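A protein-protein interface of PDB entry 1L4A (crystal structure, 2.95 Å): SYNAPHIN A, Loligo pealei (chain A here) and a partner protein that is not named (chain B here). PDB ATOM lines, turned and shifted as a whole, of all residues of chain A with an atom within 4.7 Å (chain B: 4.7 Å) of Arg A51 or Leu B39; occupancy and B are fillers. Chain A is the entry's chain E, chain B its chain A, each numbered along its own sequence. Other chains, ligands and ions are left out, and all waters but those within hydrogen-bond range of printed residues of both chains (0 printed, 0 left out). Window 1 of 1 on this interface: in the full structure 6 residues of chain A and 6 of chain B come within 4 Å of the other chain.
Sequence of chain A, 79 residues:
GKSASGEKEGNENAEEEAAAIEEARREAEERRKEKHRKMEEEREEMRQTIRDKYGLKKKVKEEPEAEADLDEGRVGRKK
The guanidinium group of Arg A47 lies within salt-bridge range of the side-chain carboxylate of Asp B42, at 2.7 Å.
The guanidinium group of Arg A47 lies close to the side-chain hydroxyl of Ser B43 (3.4 Å).
Among the printed residues, merely in contact across the chains: Arg A51 with Leu B39.
Printed residues of chain A that touch a printed residue of chain B: Arg A47 and Arg A51.
Of the 9 printed residues of chain B, 3 touch a printed residue of chain A.
Hydrophobic or aromatic side chains of chain B that line the printed part of chain A: Leu B39.
Among the printed residues, 3 pairs touch across the chains.
The backbone carbonyl oxygen (O) of Leu B39 lies within hydrogen-bond range of the side-chain hydroxyl (OG) of Ser B43.
The guanidinium group (NH1) of Arg A51 lies close to the backbone carbonyl oxygen (O) of Arg A47, 3.1 Å away.
O of Arg A51 lies within hydrogen-bond range of N of Leu A56, 3.1 Å away.
Of the printed residues of chain B, Arg A47 touches Asp B42 and Ser B43.
Arg A51 touches just one residue of chain B: Leu B39 (3.7 Å).
Lys A57 touches none of the printed residues of chain B.
Of the printed residues of chain A, Leu B39 touches Arg A51 (3.7 Å).
Printed residues of chain A within 4 Å of Asp B42: Arg A47 (2.7 Å).
Of the printed residues of chain A, Ser B43 touches Arg A47 (3.3 Å).
The nearest printed residue of chain B that does not touch Arg A51 is Ser B43 (4.9 Å).
The nearest residue of chain A that does not touch Leu B39 is Arg A47 (4.1 Å).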
ATOM      1  N   ARG A  47     -28.686  19.512 -25.371  1.00  0.00           N
ATOM      2  CA  ARG A  47     -28.126  19.040 -24.112  1.00  0.00           C
ATOM      3  C   ARG A  47     -26.893  18.170 -24.373  1.00  0.00           C
ATOM      4  O   ARG A  47     -25.798  18.489 -23.916  1.00  0.00           O
ATOM      5  CB  ARG A  47     -29.165  18.233 -23.330  1.00  0.00           C
ATOM      6  CG  ARG A  47     -30.454  18.975 -23.019  1.00  0.00           C
ATOM      7  CD  ARG A  47     -31.432  18.057 -22.298  1.00  0.00           C
ATOM      8  NE  ARG A  47     -32.781  18.609 -22.253  1.00  0.00           N
ATOM      9  CZ  ARG A  47     -33.084  19.805 -21.761  1.00  0.00           C
ATOM     10  NH1 ARG A  47     -32.127  20.582 -21.269  1.00  0.00           N
ATOM     11  NH2 ARG A  47     -34.345  20.220 -21.748  1.00  0.00           N
ATOM     12  N   GLN A  48     -27.072  17.073 -25.108  1.00  0.00           N
ATOM     13  CA  GLN A  48     -25.968  16.167 -25.416  1.00  0.00           C
ATOM     14  C   GLN A  48     -24.835  16.930 -26.091  1.00  0.00           C
ATOM     15  O   GLN A  48     -23.730  17.015 -25.557  1.00  0.00           O
ATOM     16  CB  GLN A  48     -26.450  15.034 -26.322  1.00  0.00           C
ATOM     17  N   THR A  49     -25.114  17.495 -27.263  1.00  0.00           N
ATOM     18  CA  THR A  49     -24.111  18.257 -28.000  1.00  0.00           C
ATOM     19  C   THR A  49     -23.241  19.099 -27.063  1.00  0.00           C
ATOM     20  O   THR A  49     -22.035  19.211 -27.266  1.00  0.00           O
ATOM     21  CB  THR A  49     -24.782  19.183 -29.039  1.00  0.00           C
ATOM     22  OG1 THR A  49     -23.783  19.903 -29.764  1.00  0.00           O
ATOM     23  CG2 THR A  49     -25.685  20.174 -28.367  1.00  0.00           C
ATOM     24  N   ILE A  50     -23.850  19.689 -26.041  1.00  0.00           N
ATOM     25  CA  ILE A  50     -23.112  20.514 -25.087  1.00  0.00           C
ATOM     26  C   ILE A  50     -22.442  19.615 -24.052  1.00  0.00           C
ATOM     27  O   ILE A  50     -21.253  19.752 -23.775  1.00  0.00           O
ATOM     28  CB  ILE A  50     -24.054  21.494 -24.354  1.00  0.00           C
ATOM     29  CG1 ILE A  50     -24.502  22.598 -25.315  1.00  0.00           C
ATOM     30  CG2 ILE A  50     -23.370  22.071 -23.135  1.00  0.00           C
ATOM     31  CD1 ILE A  50     -23.399  23.528 -25.745  1.00  0.00           C
ATOM     32  N   ARG A  51     -23.214  18.688 -23.493  1.00  0.00           N
ATOM     33  CA  ARG A  51     -22.732  17.773 -22.465  1.00  0.00           C
ATOM     34  C   ARG A  51     -21.498  16.985 -22.911  1.00  0.00           C
ATOM     35  O   ARG A  51     -20.571  16.773 -22.129  1.00  0.00           O
ATOM     36  CB  ARG A  51     -23.880  16.844 -22.072  1.00  0.00           C
ATOM     37  CG  ARG A  51     -23.806  16.297 -20.653  1.00  0.00           C
ATOM     38  CD  ARG A  51     -24.994  15.356 -20.329  1.00  0.00           C
ATOM     39  NE  ARG A  51     -26.144  15.984 -19.654  1.00  0.00           N
ATOM     40  CZ  ARG A  51     -27.103  16.688 -20.256  1.00  0.00           C
ATOM     41  NH1 ARG A  51     -27.071  16.876 -21.569  1.00  0.00           N
ATOM     42  NH2 ARG A  51     -28.111  17.192 -19.547  1.00  0.00           N
ATOM     43  N   ASP A  52     -21.482  16.565 -24.172  1.00  0.00           N
ATOM     44  CA  ASP A  52     -20.345  15.823 -24.713  1.00  0.00           C
ATOM     45  C   ASP A  52     -19.178  16.769 -25.000  1.00  0.00           C
ATOM     46  O   ASP A  52     -18.033  16.465 -24.696  1.00  0.00           O
ATOM     47  CB  ASP A  52     -20.757  15.098 -25.992  1.00  0.00           C
ATOM     48  N   LYS A  53     -19.490  17.922 -25.582  1.00  0.00           N
ATOM     49  CA  LYS A  53     -18.496  18.946 -25.926  1.00  0.00           C
ATOM     50  C   LYS A  53     -17.506  19.153 -24.785  1.00  0.00           C
ATOM     51  O   LYS A  53     -16.344  19.465 -25.017  1.00  0.00           O
ATOM     52  CB  LYS A  53     -19.213  20.270 -26.225  1.00  0.00           C
ATOM     53  CG  LYS A  53     -18.348  21.471 -26.540  1.00  0.00           C
ATOM     54  CD  LYS A  53     -19.234  22.688 -26.764  1.00  0.00           C
ATOM     55  CE  LYS A  53     -18.463  23.916 -27.174  1.00  0.00           C
ATOM     56  NZ  LYS A  53     -19.376  25.076 -27.306  1.00  0.00           N
ATOM     57  N   TYR A  54     -17.962  18.961 -23.553  1.00  0.00           N
ATOM     58  CA  TYR A  54     -17.095  19.159 -22.404  1.00  0.00           C
ATOM     59  C   TYR A  54     -16.723  17.887 -21.653  1.00  0.00           C
ATOM     60  O   TYR A  54     -15.770  17.883 -20.868  1.00  0.00           O
ATOM     61  CB  TYR A  54     -17.736  20.164 -21.457  1.00  0.00           C
ATOM     62  CG  TYR A  54     -17.877  21.530 -22.081  1.00  0.00           C
ATOM     63  CD1 TYR A  54     -19.099  21.965 -22.588  1.00  0.00           C
ATOM     64  CD2 TYR A  54     -16.781  22.380 -22.187  1.00  0.00           C
ATOM     65  CE1 TYR A  54     -19.231  23.217 -23.185  1.00  0.00           C
ATOM     66  CE2 TYR A  54     -16.895  23.632 -22.781  1.00  0.00           C
ATOM     67  CZ  TYR A  54     -18.126  24.045 -23.278  1.00  0.00           C
ATOM     68  OH  TYR A  54     -18.252  25.283 -23.867  1.00  0.00           O
ATOM     69  N   GLY A  55     -17.468  16.812 -21.887  1.00  0.00           N
ATOM     70  CA  GLY A  55     -17.158  15.553 -21.231  1.00  0.00           C
ATOM     71  C   GLY A  55     -17.860  15.328 -19.909  1.00  0.00           C
ATOM     72  O   GLY A  55     -17.236  15.324 -18.846  1.00  0.00           O
ATOM     73  N   LEU A  56     -19.166  15.126 -19.980  1.00  0.00           N
ATOM     74  CA  LEU A  56     -19.966  14.895 -18.789  1.00  0.00           C
ATOM     75  C   LEU A  56     -20.561  13.482 -18.846  1.00  0.00           C
ATOM     76  O   LEU A  56     -19.883  12.546 -19.292  1.00  0.00           O
ATOM     77  CB  LEU A  56     -21.047  15.978 -18.706  1.00  0.00           C
ATOM     78  CG  LEU A  56     -20.423  17.376 -18.587  1.00  0.00           C
ATOM     79  CD1 LEU A  56     -21.441  18.452 -18.893  1.00  0.00           C
ATOM     80  CD2 LEU A  56     -19.857  17.546 -17.190  1.00  0.00           C
ATOM     81  N   LYS A  57     -21.805  13.312 -18.402  1.00  0.00           N
ATOM     82  CA  LYS A  57     -22.419  11.989 -18.423  1.00  0.00           C
ATOM     83  C   LYS A  57     -23.933  12.025 -18.292  1.00  0.00           C
ATOM     84  O   LYS A  57     -24.466  13.115 -18.007  1.00  0.00           O
ATOM     85  CB  LYS A  57     -21.830  11.134 -17.311  1.00  0.00           C
ATOM     86  N   VAL B  35     -21.921  24.636 -15.934  1.00  0.00           N
ATOM     87  CA  VAL B  35     -22.507  24.269 -17.220  1.00  0.00           C
ATOM     88  C   VAL B  35     -23.424  23.079 -16.968  1.00  0.00           C
ATOM     89  O   VAL B  35     -24.533  23.002 -17.500  1.00  0.00           O
ATOM     90  CB  VAL B  35     -21.417  23.860 -18.245  1.00  0.00           C
ATOM     91  CG1 VAL B  35     -22.025  23.693 -19.635  1.00  0.00           C
ATOM     92  CG2 VAL B  35     -20.332  24.904 -18.280  1.00  0.00           C
ATOM     93  N   ASP B  36     -22.937  22.157 -16.141  1.00  0.00           N
ATOM     94  CA  ASP B  36     -23.665  20.950 -15.763  1.00  0.00           C
ATOM     95  C   ASP B  36     -24.986  21.355 -15.124  1.00  0.00           C
ATOM     96  O   ASP B  36     -26.067  21.008 -15.613  1.00  0.00           O
ATOM     97  CB  ASP B  36     -22.810  20.146 -14.775  1.00  0.00           C
ATOM     98  CG  ASP B  36     -23.597  19.076 -14.035  1.00  0.00           C
ATOM     99  OD1 ASP B  36     -24.472  19.437 -13.213  1.00  0.00           O
ATOM    100  OD2 ASP B  36     -23.332  17.874 -14.271  1.00  0.00           O
ATOM    101  N   LYS B  37     -24.883  22.103 -14.029  1.00  0.00           N
ATOM    102  CA  LYS B  37     -26.050  22.576 -13.309  1.00  0.00           C
ATOM    103  C   LYS B  37     -27.012  23.338 -14.200  1.00  0.00           C
ATOM    104  O   LYS B  37     -28.219  23.201 -14.072  1.00  0.00           O
ATOM    105  CB  LYS B  37     -25.622  23.455 -12.143  1.00  0.00           C
ATOM    106  CG  LYS B  37     -25.130  22.666 -10.952  1.00  0.00           C
ATOM    107  CD  LYS B  37     -25.377  23.435  -9.678  1.00  0.00           C
ATOM    108  CE  LYS B  37     -25.402  22.509  -8.490  1.00  0.00           C
ATOM    109  NZ  LYS B  37     -26.118  23.153  -7.354  1.00  0.00           N
ATOM    110  N   VAL B  38     -26.486  24.145 -15.107  1.00  0.00           N
ATOM    111  CA  VAL B  38     -27.353  24.900 -15.993  1.00  0.00           C
ATOM    112  C   VAL B  38     -28.076  23.916 -16.904  1.00  0.00           C
ATOM    113  O   VAL B  38     -29.046  24.275 -17.577  1.00  0.00           O
ATOM    114  CB  VAL B  38     -26.561  25.906 -16.860  1.00  0.00           C
ATOM    115  CG1 VAL B  38     -26.267  25.307 -18.223  1.00  0.00           C
ATOM    116  CG2 VAL B  38     -27.335  27.202 -16.993  1.00  0.00           C
ATOM    117  N   LEU B  39     -27.598  22.675 -16.938  1.00  0.00           N
ATOM    118  CA  LEU B  39     -28.242  21.667 -17.773  1.00  0.00           C
ATOM    119  C   LEU B  39     -29.387  21.036 -16.996  1.00  0.00           C
ATOM    120  O   LEU B  39     -30.501  20.911 -17.512  1.00  0.00           O
ATOM    121  CB  LEU B  39     -27.239  20.602 -18.230  1.00  0.00           C
ATOM    122  CG  LEU B  39     -26.305  21.061 -19.362  1.00  0.00           C
ATOM    123  CD1 LEU B  39     -25.416  19.906 -19.833  1.00  0.00           C
ATOM    124  CD2 LEU B  39     -27.149  21.596 -20.517  1.00  0.00           C
ATOM    125  N   GLU B  40     -29.123  20.645 -15.754  1.00  0.00           N
ATOM    126  CA  GLU B  40     -30.177  20.074 -14.932  1.00  0.00           C
ATOM    127  C   GLU B  40     -31.299  21.099 -14.888  1.00  0.00           C
ATOM    128  O   GLU B  40     -32.478  20.747 -14.838  1.00  0.00           O
ATOM    129  CB  GLU B  40     -29.661  19.777 -13.519  1.00  0.00           C
ATOM    130  CG  GLU B  40     -28.860  18.480 -13.429  1.00  0.00           C
ATOM    131  CD  GLU B  40     -28.242  18.247 -12.059  1.00  0.00           C
ATOM    132  OE1 GLU B  40     -28.913  18.512 -11.037  1.00  0.00           O
ATOM    133  OE2 GLU B  40     -27.083  17.784 -12.007  1.00  0.00           O
ATOM    134  N   ARG B  41     -30.914  22.373 -14.931  1.00  0.00           N
ATOM    135  CA  ARG B  41     -31.869  23.478 -14.901  1.00  0.00           C
ATOM    136  C   ARG B  41     -32.588  23.681 -16.226  1.00  0.00           C
ATOM    137  O   ARG B  41     -33.704  24.193 -16.244  1.00  0.00           O
ATOM    138  CB  ARG B  41     -31.174  24.791 -14.518  1.00  0.00           C
ATOM    139  CG  ARG B  41     -31.983  26.030 -14.903  1.00  0.00           C
ATOM    140  CD  ARG B  41     -31.408  27.337 -14.375  1.00  0.00           C
ATOM    141  NE  ARG B  41     -31.819  28.464 -15.217  1.00  0.00           N
ATOM    142  CZ  ARG B  41     -32.164  29.664 -14.758  1.00  0.00           C
ATOM    143  NH1 ARG B  41     -32.158  29.898 -13.452  1.00  0.00           N
ATOM    144  NH2 ARG B  41     -32.505  30.635 -15.605  1.00  0.00           N
ATOM    145  N   ASP B  42     -31.952  23.305 -17.332  1.00  0.00           N
ATOM    146  CA  ASP B  42     -32.575  23.474 -18.638  1.00  0.00           C
ATOM    147  C   ASP B  42     -33.666  22.422 -18.803  1.00  0.00           C
ATOM    148  O   ASP B  42     -34.684  22.658 -19.463  1.00  0.00           O
ATOM    149  CB  ASP B  42     -31.531  23.346 -19.752  1.00  0.00           C
ATOM    150  CG  ASP B  42     -32.065  23.783 -21.113  1.00  0.00           C
ATOM    151  OD1 ASP B  42     -32.932  23.077 -21.671  1.00  0.00           O
ATOM    152  OD2 ASP B  42     -31.617  24.836 -21.622  1.00  0.00           O
ATOM    153  N   SER B  43     -33.455  21.263 -18.188  1.00  0.00           N
ATOM    154  CA  SER B  43     -34.434  20.191 -18.259  1.00  0.00           C
ATOM    155  C   SER B  43     -35.595  20.545 -17.348  1.00  0.00           C
ATOM    156  O   SER B  43     -36.742  20.576 -17.794  1.00  0.00           O
ATOM    157  CB  SER B  43     -33.810  18.865 -17.829  1.00  0.00           C
ATOM    158  OG  SER B  43     -32.739  18.515 -18.691  1.00  0.00           O
